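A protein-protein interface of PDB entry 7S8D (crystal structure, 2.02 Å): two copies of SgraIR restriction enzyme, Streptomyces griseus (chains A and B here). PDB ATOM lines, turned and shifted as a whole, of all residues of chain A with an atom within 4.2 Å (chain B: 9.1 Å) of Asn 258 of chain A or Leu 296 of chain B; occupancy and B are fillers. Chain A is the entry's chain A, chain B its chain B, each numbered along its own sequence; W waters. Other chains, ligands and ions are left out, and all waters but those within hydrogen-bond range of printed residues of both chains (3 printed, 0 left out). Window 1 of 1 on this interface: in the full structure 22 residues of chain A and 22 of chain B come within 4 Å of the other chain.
Printed residues of chain B within 4 Å of Leu 254 of chain A: Tyr 255 (3.5 Å). Of the printed residues of chain B, Tyr 255 of chain A touches Tyr 251 (3.6 Å), Leu 254 (3.5 Å), Asn 258 (3.8 Å) and Ala 293 (3.6 Å). No residue of chain B comes within 4 Å of Ala 257 of chain A. Asn 258 of chain A touches just these residues of chain B: Tyr 255 (3.7 Å) and Leu 296 (3.96 Å). No residue of chain B comes within 4 Å of Val 259 of chain A. No residue of chain B comes within 4 Å of Ser 295 of chain A. Of the printed residues of chain A, Pro 183 of chain B touches Leu 296. Of the printed residues of chain A, Leu 254 of chain B touches Tyr 255 (3.5 Å). Of the printed residues of chain A, Ala 294 of chain B touches Pro 183 (3.96 Å). Leu 296 of chain B touches just these residues of chain A: Pro 183, Asn 258 and Leu 262. The nearest residue of chain B that does not touch Asn 258 of chain A is Val 259 of chain B (7.0 Å). The nearest printed residue of chain A that does not touch Ala 293 of chain B is Pro 183 of chain A (4.2 Å).
Pro 183 of chain A touches Leu 296 of chain B, and with the chains exchanged Leu 296 of chain A touches Pro 183 of chain B. Leu 254 of chain A touches Tyr 255 of chain B, and with the chains exchanged Tyr 255 of chain A touches Leu 254 of chain B. Asn 258 of chain A touches Leu 296 of chain B, and with the chains exchanged Leu 296 of chain A touches Asn 258 of chain B. Leu 262 of chain A touches Leu 296 of chain B, and with the chains exchanged Leu 296 of chain A touches Leu 262 of chain B.
Pro 183 of chain A touches Ala 294 of chain B (CG to O, 3.96 Å). Pro 183 of chain A touches Leu 296 of chain B (CG to CD2, 3.7 Å). Pro 183 of chain A touches Leu 299 of chain B. Leu 254 of chain A touches Tyr 255 of chain B (CD2 to CZ, 3.5 Å). Tyr 255 of chain A touches Leu 254 of chain B. Asn 258 of chain A touches Leu 296 of chain B (CB to CD1, 3.96 Å). Leu 262 of chain A touches Leu 296 of chain B (CD2 to O, 3.9 Å). CB of Asn 258 of chain B touches CD1 of Leu 296 of chain A (3.99 Å).
Of the 26 printed residues of chain B, 11 touch a printed residue of chain A. Printed residues of chain B that touch a printed residue of chain A: Pro 183, Tyr 251, Leu 254, Tyr 255, Asn 258, Leu 262, Ala 293, Ala 294, Leu 296, Leu 299 and Ala 300. Hydrophobic or aromatic side chains of chain B within 4 Å of the printed part of chain A: Pro 183, Tyr 251, Leu 254, Tyr 255, Leu 262, Ala 293, Leu 296, Leu 299 and Ala 300. Of the 13 printed residues of chain A, 6 touch a printed residue of chain B. Hydrophobic or aromatic side chains of chain A that line the printed part of chain B: Pro 183, Leu 254, Tyr 255, Leu 262 and Leu 296. Among the printed residues, 17 pairs touch across the chains. Among the printed residues, no Asp or Glu carboxylate lies within 4 Å of a Lys or Arg side-chain nitrogen of the other chain.
Water W3 lies within hydrogen-bond range of the side-chain hydroxyl (OH) of Tyr 255 of chain A (2.8 Å), the backbone carbonyl oxygen (O) of Ala 294 of chain B (2.9 Å) and the side-chain amide nitrogen (ND2) of Asn 258 of chain B (3.1 Å). Water W2 lies within hydrogen-bond range of the side-chain hydroxyl of Tyr 255 of chain B (2.9 Å) and the side-chain amide nitrogen of Asn 258 of chain A (3.0 Å).
The side-chain amide nitrogen (ND2) of Asn 258 of chain A is in hydrogen-bond range of the backbone carbonyl oxygen (O) of Leu 254 of chain A (2.8 Å). The side-chain amide oxygen (OD1) of Asn 258 of chain B sits at hydrogen-bond distance from the backbone NH (N) of Leu 296 of chain B (2.6 Å). OD1 of Asn 258 of chain A is in hydrogen-bond range of N of Leu 296 of chain A, 2.6 Å away.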
ATOM      1  N   PRO A 183     -27.692  28.493  31.129  1.00  0.00           N
ATOM      2  CA  PRO A 183     -26.812  28.679  32.290  1.00  0.00           C
ATOM      3  C   PRO A 183     -27.278  29.835  33.162  1.00  0.00           C
ATOM      4  O   PRO A 183     -27.678  30.892  32.667  1.00  0.00           O
ATOM      5  CB  PRO A 183     -25.444  28.962  31.657  1.00  0.00           C
ATOM      6  CG  PRO A 183     -25.528  28.371  30.286  1.00  0.00           C
ATOM      7  CD  PRO A 183     -26.954  28.553  29.856  1.00  0.00           C
ATOM      8  N   LEU A 254     -16.823  32.382  39.607  1.00  0.00           N
ATOM      9  CA  LEU A 254     -16.046  32.310  38.373  1.00  0.00           C
ATOM     10  C   LEU A 254     -16.882  31.755  37.227  1.00  0.00           C
ATOM     11  O   LEU A 254     -16.800  32.243  36.094  1.00  0.00           O
ATOM     12  CB  LEU A 254     -14.797  31.455  38.590  1.00  0.00           C
ATOM     13  CG  LEU A 254     -13.869  31.266  37.389  1.00  0.00           C
ATOM     14  CD1 LEU A 254     -13.297  32.599  36.935  1.00  0.00           C
ATOM     15  CD2 LEU A 254     -12.756  30.284  37.723  1.00  0.00           C
ATOM     16  N   TYR A 255     -17.697  30.734  37.504  1.00  0.00           N
ATOM     17  CA  TYR A 255     -18.570  30.182  36.473  1.00  0.00           C
ATOM     18  C   TYR A 255     -19.669  31.168  36.098  1.00  0.00           C
ATOM     19  O   TYR A 255     -19.909  31.423  34.912  1.00  0.00           O
ATOM     20  CB  TYR A 255     -19.172  28.859  36.952  1.00  0.00           C
ATOM     21  CG  TYR A 255     -20.295  28.344  36.078  1.00  0.00           C
ATOM     22  CD1 TYR A 255     -20.030  27.713  34.870  1.00  0.00           C
ATOM     23  CD2 TYR A 255     -21.622  28.483  36.466  1.00  0.00           C
ATOM     24  CE1 TYR A 255     -21.053  27.241  34.069  1.00  0.00           C
ATOM     25  CE2 TYR A 255     -22.653  28.014  35.673  1.00  0.00           C
ATOM     26  CZ  TYR A 255     -22.363  27.394  34.475  1.00  0.00           C
ATOM     27  OH  TYR A 255     -23.386  26.924  33.683  1.00  0.00           O
ATOM     28  N   GLU A 256     -20.346  31.737  37.098  1.00  0.00           N
ATOM     29  CA  GLU A 256     -21.442  32.659  36.822  1.00  0.00           C
ATOM     30  C   GLU A 256     -20.960  33.959  36.193  1.00  0.00           C
ATOM     31  O   GLU A 256     -21.736  34.618  35.491  1.00  0.00           O
ATOM     32  CB  GLU A 256     -22.225  32.939  38.104  1.00  0.00           C
ATOM     33  CG  GLU A 256     -22.955  31.716  38.643  1.00  0.00           C
ATOM     34  CD  GLU A 256     -23.885  32.041  39.794  1.00  0.00           C
ATOM     35  OE1 GLU A 256     -23.951  33.221  40.198  1.00  0.00           O
ATOM     36  OE2 GLU A 256     -24.552  31.111  40.294  1.00  0.00           O
ATOM     37  N   ALA A 257     -19.701  34.340  36.420  1.00  0.00           N
ATOM     38  CA  ALA A 257     -19.143  35.482  35.704  1.00  0.00           C
ATOM     39  C   ALA A 257     -19.026  35.189  34.213  1.00  0.00           C
ATOM     40  O   ALA A 257     -19.348  36.042  33.378  1.00  0.00           O
ATOM     41  CB  ALA A 257     -17.781  35.858  36.284  1.00  0.00           C
ATOM     42  N   ASN A 258     -18.564  33.986  33.862  1.00  0.00           N
ATOM     43  CA  ASN A 258     -18.508  33.598  32.457  1.00  0.00           C
ATOM     44  C   ASN A 258     -19.900  33.471  31.854  1.00  0.00           C
ATOM     45  O   ASN A 258     -20.083  33.739  30.662  1.00  0.00           O
ATOM     46  CB  ASN A 258     -17.741  32.283  32.301  1.00  0.00           C
ATOM     47  CG  ASN A 258     -16.239  32.467  32.413  1.00  0.00           C
ATOM     48  OD1 ASN A 258     -15.598  32.985  31.501  1.00  0.00           O
ATOM     49  ND2 ASN A 258     -15.670  32.033  33.533  1.00  0.00           N
ATOM     50  N   VAL A 259     -20.889  33.069  32.657  1.00  0.00           N
ATOM     51  CA  VAL A 259     -22.257  32.963  32.157  1.00  0.00           C
ATOM     52  C   VAL A 259     -22.801  34.338  31.794  1.00  0.00           C
ATOM     53  O   VAL A 259     -23.414  34.518  30.734  1.00  0.00           O
ATOM     54  CB  VAL A 259     -23.152  32.257  33.192  1.00  0.00           C
ATOM     55  CG1 VAL A 259     -24.612  32.324  32.768  1.00  0.00           C
ATOM     56  CG2 VAL A 259     -22.715  30.812  33.374  1.00  0.00           C
ATOM     57  N   MET A 260     -22.588  35.329  32.664  1.00  0.00           N
ATOM     58  CA  MET A 260     -23.062  36.679  32.378  1.00  0.00           C
ATOM     59  C   MET A 260     -22.397  37.246  31.132  1.00  0.00           C
ATOM     60  O   MET A 260     -23.048  37.914  30.321  1.00  0.00           O
ATOM     61  CB  MET A 260     -22.808  37.593  33.577  1.00  0.00           C
ATOM     62  CG  MET A 260     -23.614  37.242  34.814  1.00  0.00           C
ATOM     63  SD  MET A 260     -23.583  38.566  36.036  1.00  0.00           S
ATOM     64  CE  MET A 260     -24.380  39.882  35.119  1.00  0.00           C
ATOM     65  N   GLN A 261     -21.099  36.989  30.960  1.00  0.00           N
ATOM     66  CA  GLN A 261     -20.398  37.491  29.785  1.00  0.00           C
ATOM     67  C   GLN A 261     -20.839  36.769  28.517  1.00  0.00           C
ATOM     68  O   GLN A 261     -20.905  37.383  27.447  1.00  0.00           O
ATOM     69  CB  GLN A 261     -18.889  37.365  29.990  1.00  0.00           C
ATOM     70  CG  GLN A 261     -18.350  38.315  31.050  1.00  0.00           C
ATOM     71  CD  GLN A 261     -17.148  37.760  31.788  1.00  0.00           C
ATOM     72  OE1 GLN A 261     -16.650  36.683  31.467  1.00  0.00           O
ATOM     73  NE2 GLN A 261     -16.681  38.497  32.790  1.00  0.00           N
ATOM     74  N   LEU A 262     -21.155  35.477  28.618  1.00  0.00           N
ATOM     75  CA  LEU A 262     -21.648  34.745  27.456  1.00  0.00           C
ATOM     76  C   LEU A 262     -23.012  35.265  27.017  1.00  0.00           C
ATOM     77  O   LEU A 262     -23.256  35.456  25.821  1.00  0.00           O
ATOM     78  CB  LEU A 262     -21.708  33.247  27.771  1.00  0.00           C
ATOM     79  CG  LEU A 262     -22.091  32.234  26.682  1.00  0.00           C
ATOM     80  CD1 LEU A 262     -23.601  32.020  26.602  1.00  0.00           C
ATOM     81  CD2 LEU A 262     -21.531  32.644  25.325  1.00  0.00           C
ATOM     82  N   SER A 295     -11.792  35.313  30.317  1.00  0.00           N
ATOM     83  CA  SER A 295     -13.205  35.023  30.114  1.00  0.00           C
ATOM     84  C   SER A 295     -13.374  33.944  29.052  1.00  0.00           C
ATOM     85  O   SER A 295     -12.778  34.018  27.974  1.00  0.00           O
ATOM     86  CB  SER A 295     -13.949  36.293  29.704  1.00  0.00           C
ATOM     87  OG  SER A 295     -15.311  36.022  29.427  1.00  0.00           O
ATOM     88  N   LEU A 296     -14.191  32.935  29.364  1.00  0.00           N
ATOM     89  CA  LEU A 296     -14.362  31.816  28.443  1.00  0.00           C
ATOM     90  C   LEU A 296     -15.025  32.250  27.144  1.00  0.00           C
ATOM     91  O   LEU A 296     -14.702  31.716  26.076  1.00  0.00           O
ATOM     92  CB  LEU A 296     -15.169  30.703  29.112  1.00  0.00           C
ATOM     93  CG  LEU A 296     -14.495  30.020  30.305  1.00  0.00           C
ATOM     94  CD1 LEU A 296     -15.339  28.863  30.815  1.00  0.00           C
ATOM     95  CD2 LEU A 296     -13.097  29.548  29.933  1.00  0.00           C
ATOM     96  N   ALA A 309     -12.547  36.773  33.405  1.00  0.00           N
ATOM     97  CA  ALA A 309     -13.911  36.511  33.851  1.00  0.00           C
ATOM     98  C   ALA A 309     -14.216  37.281  35.128  1.00  0.00           C
ATOM     99  O   ALA A 309     -15.299  37.858  35.274  1.00  0.00           O
ATOM    100  CB  ALA A 309     -14.119  35.012  34.061  1.00  0.00           C
ATOM    101  N   PRO B 183      -7.390  29.322  31.351  1.00  0.00           N
ATOM    102  CA  PRO B 183      -8.275  28.568  32.247  1.00  0.00           C
ATOM    103  C   PRO B 183      -7.820  27.122  32.382  1.00  0.00           C
ATOM    104  O   PRO B 183      -7.459  26.470  31.401  1.00  0.00           O
ATOM    105  CB  PRO B 183      -9.645  28.673  31.568  1.00  0.00           C
ATOM    106  CG  PRO B 183      -9.346  29.015  30.142  1.00  0.00           C
ATOM    107  CD  PRO B 183      -8.106  29.853  30.181  1.00  0.00           C
ATOM    108  N   TYR B 251     -19.552  23.517  41.276  1.00  0.00           N
ATOM    109  CA  TYR B 251     -19.275  24.342  40.109  1.00  0.00           C
ATOM    110  C   TYR B 251     -17.861  24.199  39.566  1.00  0.00           C
ATOM    111  O   TYR B 251     -17.598  24.673  38.455  1.00  0.00           O
ATOM    112  CB  TYR B 251     -19.563  25.813  40.432  1.00  0.00           C
ATOM    113  CG  TYR B 251     -21.041  26.102  40.535  1.00  0.00           C
ATOM    114  CD1 TYR B 251     -21.771  26.483  39.418  1.00  0.00           C
ATOM    115  CD2 TYR B 251     -21.714  25.965  41.743  1.00  0.00           C
ATOM    116  CE1 TYR B 251     -23.126  26.738  39.501  1.00  0.00           C
ATOM    117  CE2 TYR B 251     -23.071  26.218  41.836  1.00  0.00           C
ATOM    118  CZ  TYR B 251     -23.771  26.604  40.711  1.00  0.00           C
ATOM    119  OH  TYR B 251     -25.121  26.857  40.793  1.00  0.00           O
ATOM    120  N   LEU B 254     -18.214  21.660  36.740  1.00  0.00           N
ATOM    121  CA  LEU B 254     -18.981  22.311  35.684  1.00  0.00           C
ATOM    122  C   LEU B 254     -18.143  23.358  34.959  1.00  0.00           C
ATOM    123  O   LEU B 254     -18.258  23.515  33.738  1.00  0.00           O
ATOM    124  CB  LEU B 254     -20.244  22.941  36.270  1.00  0.00           C
ATOM    125  CG  LEU B 254     -21.173  23.681  35.305  1.00  0.00           C
ATOM    126  CD1 LEU B 254     -21.679  22.745  34.218  1.00  0.00           C
ATOM    127  CD2 LEU B 254     -22.335  24.304  36.063  1.00  0.00           C
ATOM    128  N   TYR B 255     -17.296  24.082  35.694  1.00  0.00           N
ATOM    129  CA  TYR B 255     -16.429  25.071  35.063  1.00  0.00           C
ATOM    130  C   TYR B 255     -15.322  24.400  34.260  1.00  0.00           C
ATOM    131  O   TYR B 255     -15.066  24.766  33.108  1.00  0.00           O
ATOM    132  CB  TYR B 255     -15.839  26.005  36.120  1.00  0.00           C
ATOM    133  CG  TYR B 255     -14.719  26.883  35.608  1.00  0.00           C
ATOM    134  CD1 TYR B 255     -14.988  28.002  34.829  1.00  0.00           C
ATOM    135  CD2 TYR B 255     -13.393  26.596  35.907  1.00  0.00           C
ATOM    136  CE1 TYR B 255     -13.967  28.806  34.359  1.00  0.00           C
ATOM    137  CE2 TYR B 255     -12.367  27.396  35.442  1.00  0.00           C
ATOM    138  CZ  TYR B 255     -12.659  28.499  34.669  1.00  0.00           C
ATOM    139  OH  TYR B 255     -11.640  29.298  34.204  1.00  0.00           O
ATOM    140  N   GLU B 256     -14.650  23.410  34.855  1.00  0.00           N
ATOM    141  CA  GLU B 256     -13.571  22.719  34.160  1.00  0.00           C
ATOM    142  C   GLU B 256     -14.073  21.924  32.962  1.00  0.00           C
ATOM    143  O   GLU B 256     -13.301  21.682  32.027  1.00  0.00           O
ATOM    144  CB  GLU B 256     -12.818  21.808  35.130  1.00  0.00           C
ATOM    145  CG  GLU B 256     -12.064  22.572  36.212  1.00  0.00           C
ATOM    146  CD  GLU B 256     -11.179  21.680  37.061  1.00  0.00           C
ATOM    147  OE1 GLU B 256     -11.121  20.462  36.795  1.00  0.00           O
ATOM    148  OE2 GLU B 256     -10.537  22.203  37.996  1.00  0.00           O
ATOM    149  N   ALA B 257     -15.344  21.516  32.965  1.00  0.00           N
ATOM    150  CA  ALA B 257     -15.922  20.899  31.777  1.00  0.00           C
ATOM    151  C   ALA B 257     -15.991  21.892  30.625  1.00  0.00           C
ATOM    152  O   ALA B 257     -15.647  21.559  29.484  1.00  0.00           O
ATOM    153  CB  ALA B 257     -17.312  20.349  32.093  1.00  0.00           C
ATOM    154  N   ASN B 258     -16.431  23.122  30.906  1.00  0.00           N
ATOM    155  CA  ASN B 258     -16.478  24.149  29.872  1.00  0.00           C
ATOM    156  C   ASN B 258     -15.083  24.542  29.407  1.00  0.00           C
ATOM    157  O   ASN B 258     -14.901  24.903  28.239  1.00  0.00           O
ATOM    158  CB  ASN B 258     -17.234  25.376  30.385  1.00  0.00           C
ATOM    159  CG  ASN B 258     -18.736  25.165  30.417  1.00  0.00           C
ATOM    160  OD1 ASN B 258     -19.403  25.238  29.385  1.00  0.00           O
ATOM    161  ND2 ASN B 258     -19.275  24.909  31.603  1.00  0.00           N
ATOM    162  N   VAL B 259     -14.091  24.483  30.299  1.00  0.00           N
ATOM    163  CA  VAL B 259     -12.723  24.812  29.911  1.00  0.00           C
ATOM    164  C   VAL B 259     -12.190  23.791  28.915  1.00  0.00           C
ATOM    165  O   VAL B 259     -11.582  24.152  27.900  1.00  0.00           O
ATOM    166  CB  VAL B 259     -11.821  24.915  31.154  1.00  0.00           C
ATOM    167  CG1 VAL B 259     -10.364  25.068  30.743  1.00  0.00           C
ATOM    168  CG2 VAL B 259     -12.254  26.081  32.029  1.00  0.00           C
ATOM    169  N   GLN B 261     -13.912  21.878  26.885  1.00  0.00           N
ATOM    170  CA  GLN B 261     -14.610  22.032  25.614  1.00  0.00           C
ATOM    171  C   GLN B 261     -14.156  23.290  24.883  1.00  0.00           C
ATOM    172  O   GLN B 261     -14.071  23.300  23.650  1.00  0.00           O
ATOM    173  CB  GLN B 261     -16.118  22.048  25.850  1.00  0.00           C
ATOM    174  CG  GLN B 261     -16.668  20.705  26.302  1.00  0.00           C
ATOM    175  CD  GLN B 261     -17.873  20.833  27.210  1.00  0.00           C
ATOM    176  OE1 GLN B 261     -18.352  21.936  27.475  1.00  0.00           O
ATOM    177  NE2 GLN B 261     -18.368  19.703  27.699  1.00  0.00           N
ATOM    178  N   LEU B 262     -13.852  24.357  25.625  1.00  0.00           N
ATOM    179  CA  LEU B 262     -13.358  25.575  24.992  1.00  0.00           C
ATOM    180  C   LEU B 262     -11.997  25.347  24.343  1.00  0.00           C
ATOM    181  O   LEU B 262     -11.759  25.790  23.214  1.00  0.00           O
ATOM    182  CB  LEU B 262     -13.291  26.705  26.023  1.00  0.00           C
ATOM    183  CG  LEU B 262     -12.891  28.123  25.592  1.00  0.00           C
ATOM    184  CD1 LEU B 262     -11.382  28.337  25.663  1.00  0.00           C
ATOM    185  CD2 LEU B 262     -13.416  28.441  24.200  1.00  0.00           C
ATOM    186  N   GLU B 265     -12.543  21.647  21.706  1.00  0.00           N
ATOM    187  CA  GLU B 265     -13.461  21.861  20.591  1.00  0.00           C
ATOM    188  C   GLU B 265     -13.227  23.208  19.919  1.00  0.00           C
ATOM    189  O   GLU B 265     -13.383  23.325  18.698  1.00  0.00           O
ATOM    190  CB  GLU B 265     -14.911  21.757  21.066  1.00  0.00           C
ATOM    191  CG  GLU B 265     -15.279  20.421  21.689  1.00  0.00           C
ATOM    192  CD  GLU B 265     -16.720  20.376  22.163  1.00  0.00           C
ATOM    193  OE1 GLU B 265     -17.380  21.436  22.168  1.00  0.00           O
ATOM    194  OE2 GLU B 265     -17.195  19.280  22.529  1.00  0.00           O
ATOM    195  N   ALA B 293     -27.068  22.458  32.260  1.00  0.00           N
ATOM    196  CA  ALA B 293     -26.685  23.655  31.526  1.00  0.00           C
ATOM    197  C   ALA B 293     -25.917  23.300  30.259  1.00  0.00           C
ATOM    198  O   ALA B 293     -25.085  22.389  30.248  1.00  0.00           O
ATOM    199  CB  ALA B 293     -25.838  24.569  32.409  1.00  0.00           C
ATOM    200  N   ALA B 294     -26.205  24.033  29.187  1.00  0.00           N
ATOM    201  CA  ALA B 294     -25.500  23.838  27.932  1.00  0.00           C
ATOM    202  C   ALA B 294     -24.053  24.305  28.055  1.00  0.00           C
ATOM    203  O   ALA B 294     -23.706  25.134  28.901  1.00  0.00           O
ATOM    204  CB  ALA B 294     -26.201  24.589  26.800  1.00  0.00           C
ATOM    205  N   SER B 295     -23.202  23.754  27.191  1.00  0.00           N
ATOM    206  CA  SER B 295     -21.794  24.125  27.181  1.00  0.00           C
ATOM    207  C   SER B 295     -21.640  25.582  26.764  1.00  0.00           C
ATOM    208  O   SER B 295     -22.260  26.031  25.795  1.00  0.00           O
ATOM    209  CB  SER B 295     -21.014  23.216  26.235  1.00  0.00           C
ATOM    210  OG  SER B 295     -19.642  23.574  26.194  1.00  0.00           O
ATOM    211  N   LEU B 296     -20.803  26.321  27.498  1.00  0.00           N
ATOM    212  CA  LEU B 296     -20.648  27.747  27.227  1.00  0.00           C
ATOM    213  C   LEU B 296     -20.009  27.991  25.864  1.00  0.00           C
ATOM    214  O   LEU B 296     -20.392  28.929  25.155  1.00  0.00           O
ATOM    215  CB  LEU B 296     -19.828  28.408  28.334  1.00  0.00           C
ATOM    216  CG  LEU B 296     -20.448  28.369  29.733  1.00  0.00           C
ATOM    217  CD1 LEU B 296     -19.619  29.184  30.715  1.00  0.00           C
ATOM    218  CD2 LEU B 296     -21.887  28.864  29.697  1.00  0.00           C
ATOM    219  N   TYR B 297     -19.037  27.161  25.476  1.00  0.00           N
ATOM    220  CA  TYR B 297     -18.426  27.333  24.162  1.00  0.00           C
ATOM    221  C   TYR B 297     -19.418  27.035  23.046  1.00  0.00           C
ATOM    222  O   TYR B 297     -19.459  27.751  22.039  1.00  0.00           O
ATOM    223  CB  TYR B 297     -17.192  26.445  24.011  1.00  0.00           C
ATOM    224  CG  TYR B 297     -16.752  26.338  22.570  1.00  0.00           C
ATOM    225  CD1 TYR B 297     -16.111  27.398  21.942  1.00  0.00           C
ATOM    226  CD2 TYR B 297     -17.006  25.192  21.826  1.00  0.00           C
ATOM    227  CE1 TYR B 297     -15.722  27.316  20.621  1.00  0.00           C
ATOM    228  CE2 TYR B 297     -16.621  25.100  20.503  1.00  0.00           C
ATOM    229  CZ  TYR B 297     -15.981  26.166  19.905  1.00  0.00           C
ATOM    230  OH  TYR B 297     -15.591  26.079  18.588  1.00  0.00           O
ATOM    231  N   GLY B 298     -20.212  25.972  23.199  1.00  0.00           N
ATOM    232  CA  GLY B 298     -21.186  25.636  22.174  1.00  0.00           C
ATOM    233  C   GLY B 298     -22.186  26.751  21.933  1.00  0.00           C
ATOM    234  O   GLY B 298     -22.601  26.992  20.796  1.00  0.00           O
ATOM    235  N   LEU B 299     -22.582  27.450  22.998  1.00  0.00           N
ATOM    236  CA  LEU B 299     -23.468  28.597  22.841  1.00  0.00           C
ATOM    237  C   LEU B 299     -22.756  29.764  22.170  1.00  0.00           C
ATOM    238  O   LEU B 299     -23.375  30.510  21.402  1.00  0.00           O
ATOM    239  CB  LEU B 299     -24.022  29.025  24.200  1.00  0.00           C
ATOM    240  CG  LEU B 299     -24.793  27.965  24.988  1.00  0.00           C
ATOM    241  CD1 LEU B 299     -25.305  28.539  26.301  1.00  0.00           C
ATOM    242  CD2 LEU B 299     -25.936  27.403  24.158  1.00  0.00           C
ATOM    243  N   ALA B 300     -21.461  29.935  22.441  1.00  0.00           N
ATOM    244  CA  ALA B 300     -20.718  31.035  21.835  1.00  0.00           C
ATOM    245  C   ALA B 300     -20.473  30.788  20.352  1.00  0.00           C
ATOM    246  O   ALA B 300     -20.581  31.713  19.538  1.00  0.00           O
ATOM    247  CB  ALA B 300     -19.395  31.245  22.570  1.00  0.00           C
ATOM    248  N   GLU B 301     -20.138  29.549  19.981  1.00  0.00           N
ATOM    249  CA  GLU B 301     -19.910  29.238  18.573  1.00  0.00           C
ATOM    250  C   GLU B 301     -21.200  29.346  17.767  1.00  0.00           C
ATOM    251  O   GLU B 301     -21.196  29.870  16.648  1.00  0.00           O
ATOM    252  CB  GLU B 301     -19.305  27.841  18.435  1.00  0.00           C
ATOM    253  N   GLY B 302     -22.309  28.858  18.320  1.00  0.00           N
ATOM    254  CA  GLY B 302     -23.586  28.951  17.643  1.00  0.00           C
ATOM    255  C   GLY B 302     -23.701  28.144  16.372  1.00  0.00           C
ATOM    256  O   GLY B 302     -24.514  28.481  15.508  1.00  0.00           O
ATOM    257  N   VAL B 306     -25.406  21.934  19.931  1.00  0.00           N
ATOM    258  CA  VAL B 306     -24.876  22.216  21.259  1.00  0.00           C
ATOM    259  C   VAL B 306     -25.210  21.058  22.188  1.00  0.00           C
ATOM    260  O   VAL B 306     -26.330  20.534  22.175  1.00  0.00           O
ATOM    261  CB  VAL B 306     -25.441  23.545  21.799  1.00  0.00           C
ATOM    262  CG1 VAL B 306     -24.979  23.788  23.230  1.00  0.00           C
ATOM    263  CG2 VAL B 306     -25.031  24.700  20.898  1.00  0.00           C
ATOM    264  N   HIS B 307     -24.232  20.649  22.990  1.00  0.00           N
ATOM    265  CA  HIS B 307     -24.426  19.643  24.022  1.00  0.00           C
ATOM    266  C   HIS B 307     -24.146  20.260  25.387  1.00  0.00           C
ATOM    267  O   HIS B 307     -23.603  21.363  25.499  1.00  0.00           O
ATOM    268  CB  HIS B 307     -23.530  18.419  23.783  1.00  0.00           C
ATOM    269  CG  HIS B 307     -22.064  18.722  23.808  1.00  0.00           C
ATOM    270  ND1 HIS B 307     -21.345  18.832  24.979  1.00  0.00           N
ATOM    271  CD2 HIS B 307     -21.178  18.932  22.805  1.00  0.00           C
ATOM    272  CE1 HIS B 307     -20.082  19.099  24.696  1.00  0.00           C
ATOM    273  NE2 HIS B 307     -19.955  19.164  23.384  1.00  0.00           N
ATOM    274  N   ARG B 308     -24.534  19.537  26.434  1.00  0.00           N
ATOM    275  CA  ARG B 308     -24.338  20.024  27.791  1.00  0.00           C
ATOM    276  C   ARG B 308     -22.852  20.091  28.133  1.00  0.00           C
ATOM    277  O   ARG B 308     -22.017  19.402  27.543  1.00  0.00           O
ATOM    278  CB  ARG B 308     -25.056  19.124  28.797  1.00  0.00           C
ATOM    279  CG  ARG B 308     -26.570  19.120  28.680  1.00  0.00           C
ATOM    280  CD  ARG B 308     -27.192  18.189  29.709  1.00  0.00           C
ATOM    281  NE  ARG B 308     -28.647  18.168  29.627  1.00  0.00           N
ATOM    282  CZ  ARG B 308     -29.427  17.409  30.385  1.00  0.00           C
ATOM    283  NH1 ARG B 308     -28.924  16.591  31.294  1.00  0.00           N
ATOM    284  NH2 ARG B 308     -30.747  17.472  30.224  1.00  0.00           N
ATOM    285  N   ALA B 309     -22.528  20.950  29.102  1.00  0.00           N
ATOM    286  CA  ALA B 309     -21.171  20.973  29.638  1.00  0.00           C
ATOM    287  C   ALA B 309     -20.849  19.656  30.333  1.00  0.00           C
ATOM    288  O   ALA B 309     -19.786  19.065  30.114  1.00  0.00           O
ATOM    289  CB  ALA B 309     -21.005  22.152  30.597  1.00  0.00           C
ATOM    290  N   ILE B 310     -21.764  19.182  31.173  1.00  0.00           N
ATOM    291  CA  ILE B 310     -21.685  17.861  31.783  1.00  0.00           C
ATOM    292  C   ILE B 310     -22.838  17.039  31.226  1.00  0.00           C
ATOM    293  O   ILE B 310     -24.009  17.392  31.416  1.00  0.00           O
ATOM    294  CB  ILE B 310     -21.742  17.939  33.316  1.00  0.00           C
ATOM    295  CG1 ILE B 310     -20.520  18.687  33.854  1.00  0.00           C
ATOM    296  CG2 ILE B 310     -21.834  16.546  33.919  1.00  0.00           C
ATOM    297  CD1 ILE B 310     -20.493  18.812  35.359  1.00  0.00           C
HETATM  298  O   HOH W   1     -25.330  28.796  38.610  1.00  0.00           O
HETATM  299  O   HOH W   2     -12.688  31.738  33.015  1.00  0.00           O
HETATM  300  O   HOH W   3     -22.353  25.466  31.479  1.00  0.00           O
